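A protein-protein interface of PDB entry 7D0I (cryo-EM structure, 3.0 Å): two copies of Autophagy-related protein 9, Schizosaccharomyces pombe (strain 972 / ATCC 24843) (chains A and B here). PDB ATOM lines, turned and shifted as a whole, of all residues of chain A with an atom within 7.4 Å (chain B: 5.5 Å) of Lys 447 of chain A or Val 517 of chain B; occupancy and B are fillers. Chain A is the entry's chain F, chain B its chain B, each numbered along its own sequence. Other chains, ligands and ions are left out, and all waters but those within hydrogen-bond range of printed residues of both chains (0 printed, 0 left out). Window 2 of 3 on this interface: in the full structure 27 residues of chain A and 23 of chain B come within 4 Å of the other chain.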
ATOM      1  N   TYR A 441      17.291  -3.241   0.980  1.00  0.00           N
ATOM      2  CA  TYR A 441      17.454  -2.429   2.174  1.00  0.00           C
ATOM      3  C   TYR A 441      18.460  -2.971   3.178  1.00  0.00           C
ATOM      4  O   TYR A 441      18.716  -2.298   4.180  1.00  0.00           O
ATOM      5  CB  TYR A 441      16.101  -2.245   2.871  1.00  0.00           C
ATOM      6  CG  TYR A 441      15.146  -1.353   2.121  1.00  0.00           C
ATOM      7  CD1 TYR A 441      15.301   0.022   2.135  1.00  0.00           C
ATOM      8  CD2 TYR A 441      14.088  -1.884   1.405  1.00  0.00           C
ATOM      9  CE1 TYR A 441      14.431   0.839   1.454  1.00  0.00           C
ATOM     10  CE2 TYR A 441      13.213  -1.071   0.723  1.00  0.00           C
ATOM     11  CZ  TYR A 441      13.390   0.290   0.751  1.00  0.00           C
ATOM     12  OH  TYR A 441      12.520   1.106   0.071  1.00  0.00           O
ATOM     13  N   PHE A 442      19.038  -4.154   2.958  1.00  0.00           N
ATOM     14  CA  PHE A 442      19.993  -4.675   3.930  1.00  0.00           C
ATOM     15  C   PHE A 442      21.217  -3.777   4.035  1.00  0.00           C
ATOM     16  O   PHE A 442      21.693  -3.486   5.138  1.00  0.00           O
ATOM     17  CB  PHE A 442      20.407  -6.094   3.553  1.00  0.00           C
ATOM     18  CG  PHE A 442      21.440  -6.680   4.463  1.00  0.00           C
ATOM     19  CD1 PHE A 442      21.077  -7.223   5.681  1.00  0.00           C
ATOM     20  CD2 PHE A 442      22.773  -6.688   4.102  1.00  0.00           C
ATOM     21  CE1 PHE A 442      22.025  -7.764   6.521  1.00  0.00           C
ATOM     22  CE2 PHE A 442      23.723  -7.227   4.939  1.00  0.00           C
ATOM     23  CZ  PHE A 442      23.349  -7.765   6.151  1.00  0.00           C
ATOM     24  N   ASN A 443      21.734  -3.329   2.891  1.00  0.00           N
ATOM     25  CA  ASN A 443      22.908  -2.465   2.887  1.00  0.00           C
ATOM     26  C   ASN A 443      22.669  -1.215   3.727  1.00  0.00           C
ATOM     27  O   ASN A 443      23.464  -0.885   4.615  1.00  0.00           O
ATOM     28  CB  ASN A 443      23.266  -2.095   1.449  1.00  0.00           C
ATOM     29  CG  ASN A 443      24.618  -1.436   1.341  1.00  0.00           C
ATOM     30  OD1 ASN A 443      25.504  -1.677   2.159  1.00  0.00           O
ATOM     31  ND2 ASN A 443      24.787  -0.597   0.328  1.00  0.00           N
ATOM     32  N   GLU A 444      21.561  -0.520   3.476  1.00  0.00           N
ATOM     33  CA  GLU A 444      21.310   0.735   4.169  1.00  0.00           C
ATOM     34  C   GLU A 444      20.946   0.522   5.630  1.00  0.00           C
ATOM     35  O   GLU A 444      21.314   1.339   6.478  1.00  0.00           O
ATOM     36  CB  GLU A 444      20.204   1.518   3.460  1.00  0.00           C
ATOM     37  CG  GLU A 444      20.627   2.146   2.140  1.00  0.00           C
ATOM     38  CD  GLU A 444      20.895   1.119   1.050  1.00  0.00           C
ATOM     39  OE1 GLU A 444      20.449  -0.038   1.199  1.00  0.00           O
ATOM     40  OE2 GLU A 444      21.555   1.468   0.051  1.00  0.00           O
ATOM     41  N   TYR A 445      20.239  -0.555   5.954  1.00  0.00           N
ATOM     42  CA  TYR A 445      19.783  -0.768   7.319  1.00  0.00           C
ATOM     43  C   TYR A 445      20.789  -1.521   8.178  1.00  0.00           C
ATOM     44  O   TYR A 445      20.520  -1.745   9.363  1.00  0.00           O
ATOM     45  CB  TYR A 445      18.441  -1.508   7.316  1.00  0.00           C
ATOM     46  CG  TYR A 445      17.255  -0.610   7.032  1.00  0.00           C
ATOM     47  CD1 TYR A 445      16.406  -0.213   8.049  1.00  0.00           C
ATOM     48  CD2 TYR A 445      16.998  -0.155   5.750  1.00  0.00           C
ATOM     49  CE1 TYR A 445      15.328   0.607   7.800  1.00  0.00           C
ATOM     50  CE2 TYR A 445      15.922   0.665   5.489  1.00  0.00           C
ATOM     51  CZ  TYR A 445      15.091   1.043   6.517  1.00  0.00           C
ATOM     52  OH  TYR A 445      14.019   1.864   6.262  1.00  0.00           O
ATOM     53  N   HIS A 446      21.929  -1.927   7.621  1.00  0.00           N
ATOM     54  CA  HIS A 446      23.016  -2.422   8.449  1.00  0.00           C
ATOM     55  C   HIS A 446      24.300  -1.612   8.322  1.00  0.00           C
ATOM     56  O   HIS A 446      25.231  -1.846   9.102  1.00  0.00           O
ATOM     57  CB  HIS A 446      23.319  -3.893   8.131  1.00  0.00           C
ATOM     58  CG  HIS A 446      23.997  -4.623   9.251  1.00  0.00           C
ATOM     59  ND1 HIS A 446      25.342  -4.495   9.516  1.00  0.00           N
ATOM     60  CD2 HIS A 446      23.509  -5.484  10.176  1.00  0.00           C
ATOM     61  CE1 HIS A 446      25.656  -5.248  10.555  1.00  0.00           C
ATOM     62  NE2 HIS A 446      24.563  -5.857  10.974  1.00  0.00           N
ATOM     63  N   LYS A 447      24.385  -0.678   7.374  1.00  0.00           N
ATOM     64  CA  LYS A 447      25.559   0.177   7.237  1.00  0.00           C
ATOM     65  C   LYS A 447      25.204   1.657   7.268  1.00  0.00           C
ATOM     66  O   LYS A 447      26.052   2.496   6.944  1.00  0.00           O
ATOM     67  CB  LYS A 447      26.318  -0.153   5.946  1.00  0.00           C
ATOM     68  CG  LYS A 447      27.165  -1.418   6.018  1.00  0.00           C
ATOM     69  CD  LYS A 447      26.327  -2.677   5.887  1.00  0.00           C
ATOM     70  CE  LYS A 447      26.996  -3.851   6.570  1.00  0.00           C
ATOM     71  NZ  LYS A 447      26.073  -5.007   6.677  1.00  0.00           N
ATOM     72  N   ASN A 448      23.973   1.996   7.641  1.00  0.00           N
ATOM     73  CA  ASN A 448      23.539   3.380   7.778  1.00  0.00           C
ATOM     74  C   ASN A 448      22.305   3.431   8.671  1.00  0.00           C
ATOM     75  O   ASN A 448      21.199   3.688   8.180  1.00  0.00           O
ATOM     76  CB  ASN A 448      23.243   3.992   6.409  1.00  0.00           C
ATOM     77  CG  ASN A 448      22.817   5.445   6.497  1.00  0.00           C
ATOM     78  OD1 ASN A 448      23.122   6.134   7.467  1.00  0.00           O
ATOM     79  ND2 ASN A 448      22.106   5.915   5.481  1.00  0.00           N
ATOM     80  N   PRO A 449      22.444   3.183   9.975  1.00  0.00           N
ATOM     81  CA  PRO A 449      21.261   3.186  10.852  1.00  0.00           C
ATOM     82  C   PRO A 449      20.563   4.530  10.934  1.00  0.00           C
ATOM     83  O   PRO A 449      19.418   4.581  11.398  1.00  0.00           O
ATOM     84  CB  PRO A 449      21.831   2.769  12.213  1.00  0.00           C
ATOM     85  CG  PRO A 449      23.081   2.026  11.883  1.00  0.00           C
ATOM     86  CD  PRO A 449      23.649   2.736  10.691  1.00  0.00           C
ATOM     87  N   GLY A 450      21.208   5.616  10.502  1.00  0.00           N
ATOM     88  CA  GLY A 450      20.525   6.897  10.450  1.00  0.00           C
ATOM     89  C   GLY A 450      19.296   6.870   9.566  1.00  0.00           C
ATOM     90  O   GLY A 450      18.312   7.560   9.842  1.00  0.00           O
ATOM     91  N   PHE B 512      24.556  -7.429  -4.475  1.00  0.00           N
ATOM     92  CA  PHE B 512      25.890  -8.025  -4.405  1.00  0.00           C
ATOM     93  C   PHE B 512      26.535  -7.764  -3.051  1.00  0.00           C
ATOM     94  O   PHE B 512      27.080  -8.679  -2.421  1.00  0.00           O
ATOM     95  CB  PHE B 512      26.777  -7.481  -5.523  1.00  0.00           C
ATOM     96  CG  PHE B 512      26.446  -8.017  -6.880  1.00  0.00           C
ATOM     97  CD1 PHE B 512      25.814  -9.233  -7.024  1.00  0.00           C
ATOM     98  CD2 PHE B 512      26.774  -7.301  -8.014  1.00  0.00           C
ATOM     99  CE1 PHE B 512      25.512  -9.721  -8.275  1.00  0.00           C
ATOM    100  CE2 PHE B 512      26.475  -7.783  -9.264  1.00  0.00           C
ATOM    101  CZ  PHE B 512      25.844  -8.994  -9.396  1.00  0.00           C
ATOM    102  N   THR B 513      26.487  -6.514  -2.590  1.00  0.00           N
ATOM    103  CA  THR B 513      27.122  -6.158  -1.327  1.00  0.00           C
ATOM    104  C   THR B 513      26.453  -6.858  -0.155  1.00  0.00           C
ATOM    105  O   THR B 513      27.127  -7.262   0.797  1.00  0.00           O
ATOM    106  CB  THR B 513      27.089  -4.640  -1.146  1.00  0.00           C
ATOM    107  OG1 THR B 513      27.947  -4.027  -2.114  1.00  0.00           O
ATOM    108  CG2 THR B 513      27.546  -4.249   0.246  1.00  0.00           C
ATOM    109  N   ALA B 514      25.131  -7.008  -0.202  1.00  0.00           N
ATOM    110  CA  ALA B 514      24.434  -7.727   0.858  1.00  0.00           C
ATOM    111  C   ALA B 514      24.911  -9.169   0.930  1.00  0.00           C
ATOM    112  O   ALA B 514      25.201  -9.685   2.015  1.00  0.00           O
ATOM    113  CB  ALA B 514      22.926  -7.666   0.624  1.00  0.00           C
ATOM    114  N   ILE B 515      25.011  -9.830  -0.224  1.00  0.00           N
ATOM    115  CA  ILE B 515      25.507 -11.205  -0.232  1.00  0.00           C
ATOM    116  C   ILE B 515      26.932 -11.265   0.305  1.00  0.00           C
ATOM    117  O   ILE B 515      27.271 -12.139   1.113  1.00  0.00           O
ATOM    118  CB  ILE B 515      25.406 -11.806  -1.643  1.00  0.00           C
ATOM    119  CG1 ILE B 515      24.034 -12.441  -1.836  1.00  0.00           C
ATOM    120  CG2 ILE B 515      26.490 -12.840  -1.867  1.00  0.00           C
ATOM    121  CD1 ILE B 515      23.778 -13.600  -0.911  1.00  0.00           C
ATOM    122  N   LEU B 516      27.784 -10.330  -0.120  1.00  0.00           N
ATOM    123  CA  LEU B 516      29.179 -10.372   0.305  1.00  0.00           C
ATOM    124  C   LEU B 516      29.315 -10.152   1.805  1.00  0.00           C
ATOM    125  O   LEU B 516      30.085 -10.851   2.471  1.00  0.00           O
ATOM    126  CB  LEU B 516      30.003  -9.339  -0.466  1.00  0.00           C
ATOM    127  CG  LEU B 516      30.134  -9.589  -1.967  1.00  0.00           C
ATOM    128  CD1 LEU B 516      31.131  -8.628  -2.591  1.00  0.00           C
ATOM    129  CD2 LEU B 516      30.525 -11.029  -2.241  1.00  0.00           C
ATOM    130  N   VAL B 517      28.573  -9.196   2.359  1.00  0.00           N
ATOM    131  CA  VAL B 517      28.675  -8.929   3.789  1.00  0.00           C
ATOM    132  C   VAL B 517      28.086 -10.080   4.591  1.00  0.00           C
ATOM    133  O   VAL B 517      28.614 -10.448   5.647  1.00  0.00           O
ATOM    134  CB  VAL B 517      28.005  -7.589   4.137  1.00  0.00           C
ATOM    135  CG1 VAL B 517      27.981  -7.390   5.636  1.00  0.00           C
ATOM    136  CG2 VAL B 517      28.743  -6.447   3.476  1.00  0.00           C
ATOM    137  N   ILE B 518      26.999 -10.681   4.105  1.00  0.00           N
ATOM    138  CA  ILE B 518      26.412 -11.806   4.828  1.00  0.00           C
ATOM    139  C   ILE B 518      27.222 -13.081   4.671  1.00  0.00           C
ATOM    140  O   ILE B 518      27.012 -14.034   5.431  1.00  0.00           O
ATOM    141  CB  ILE B 518      24.956 -12.034   4.379  1.00  0.00           C
ATOM    142  CG1 ILE B 518      24.143 -12.646   5.519  1.00  0.00           C
ATOM    143  CG2 ILE B 518      24.905 -12.928   3.154  1.00  0.00           C
ATOM    144  CD1 ILE B 518      22.667 -12.751   5.223  1.00  0.00           C
ATOM    145  N   ILE B 519      28.144 -13.130   3.709  1.00  0.00           N
ATOM    146  CA  ILE B 519      29.033 -14.280   3.581  1.00  0.00           C
ATOM    147  C   ILE B 519      30.384 -14.060   4.258  1.00  0.00           C
ATOM    148  O   ILE B 519      31.065 -15.046   4.581  1.00  0.00           O
ATOM    149  CB  ILE B 519      29.236 -14.664   2.100  1.00  0.00           C
ATOM    150  CG1 ILE B 519      29.543 -16.155   1.975  1.00  0.00           C
ATOM    151  CG2 ILE B 519      30.359 -13.858   1.478  1.00  0.00           C
ATOM    152  CD1 ILE B 519      28.437 -17.048   2.489  1.00  0.00           C
ATOM    153  N   THR B 520      30.793 -12.809   4.486  1.00  0.00           N
ATOM    154  CA  THR B 520      32.038 -12.563   5.201  1.00  0.00           C
ATOM    155  C   THR B 520      31.867 -12.624   6.710  1.00  0.00           C
ATOM    156  O   THR B 520      32.864 -12.745   7.428  1.00  0.00           O
ATOM    157  CB  THR B 520      32.628 -11.207   4.819  1.00  0.00           C
ATOM    158  OG1 THR B 520      31.646 -10.182   5.011  1.00  0.00           O
ATOM    159  CG2 THR B 520      33.090 -11.213   3.372  1.00  0.00           C
ATOM    160  N   VAL B 521      30.629 -12.538   7.210  1.00  0.00           N
ATOM    161  CA  VAL B 521      30.382 -12.758   8.632  1.00  0.00           C
ATOM    162  C   VAL B 521      30.360 -14.232   8.989  1.00  0.00           C
ATOM    163  O   VAL B 521      30.168 -14.576  10.162  1.00  0.00           O
ATOM    164  CB  VAL B 521      29.063 -12.094   9.073  1.00  0.00           C
ATOM    165  CG1 VAL B 521      29.173 -10.582   8.968  1.00  0.00           C
ATOM    166  CG2 VAL B 521      27.911 -12.610   8.236  1.00  0.00           C
ATOM    167  N   LEU B 542      34.108  -5.294  -2.295  1.00  0.00           N
ATOM    168  CA  LEU B 542      33.242  -4.601  -1.349  1.00  0.00           C
ATOM    169  C   LEU B 542      33.516  -3.103  -1.360  1.00  0.00           C
ATOM    170  O   LEU B 542      32.582  -2.294  -1.369  1.00  0.00           O
ATOM    171  CB  LEU B 542      33.435  -5.175   0.054  1.00  0.00           C
ATOM    172  CG  LEU B 542      32.265  -4.995   1.020  1.00  0.00           C
ATOM    173  CD1 LEU B 542      31.058  -5.747   0.506  1.00  0.00           C
ATOM    174  CD2 LEU B 542      32.639  -5.475   2.405  1.00  0.00           C
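No position is printed for both chains. Of the 3 pairs that touch across the chains among the printed residues, none has its exchanged pair printed and touching as well.
The backbone carbonyl oxygen (O) of Val 517 of chain B lies within hydrogen-bond range of the side-chain hydroxyl (OG1) of Thr 520 of chain B, 3.1 Å away. A ring nitrogen (ND1) of His 446 of chain A is in hydrogen-bond range of the side-chain amino group (NZ) of Lys 447 of chain A (3.0 Å).
Lys 447 of chain A touches just one residue of chain B: Val 517 (3.2 Å). Val 517 of chain B touches just one residue of chain A: Lys 447 (3.2 Å). Printed residues of chain A within 4 Å of Ala 514 of chain B: Phe 442 (3.6 Å). Of the printed residues of chain B, Asn 443 of chain A touches Thr 513 (3.8 Å). The nearest printed residue of chain A that does not touch Thr 513 of chain B is Phe 442 of chain A (5.4 Å).
Hydrophobic or aromatic side chains of chain B that line the printed part of chain A: Ala 514 and Val 517. Among the printed residues, no Asp or Glu carboxylate lies within 4 Å of a Lys or Arg side-chain nitrogen of the other chain.
Among the printed residues, pairs that only touch across the chains: Phe 442 of chain A with Ala 514 of chain B, Asn 443 of chain A with Thr 513 of chain B and Lys 447 of chain A with Val 517 of chain B.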
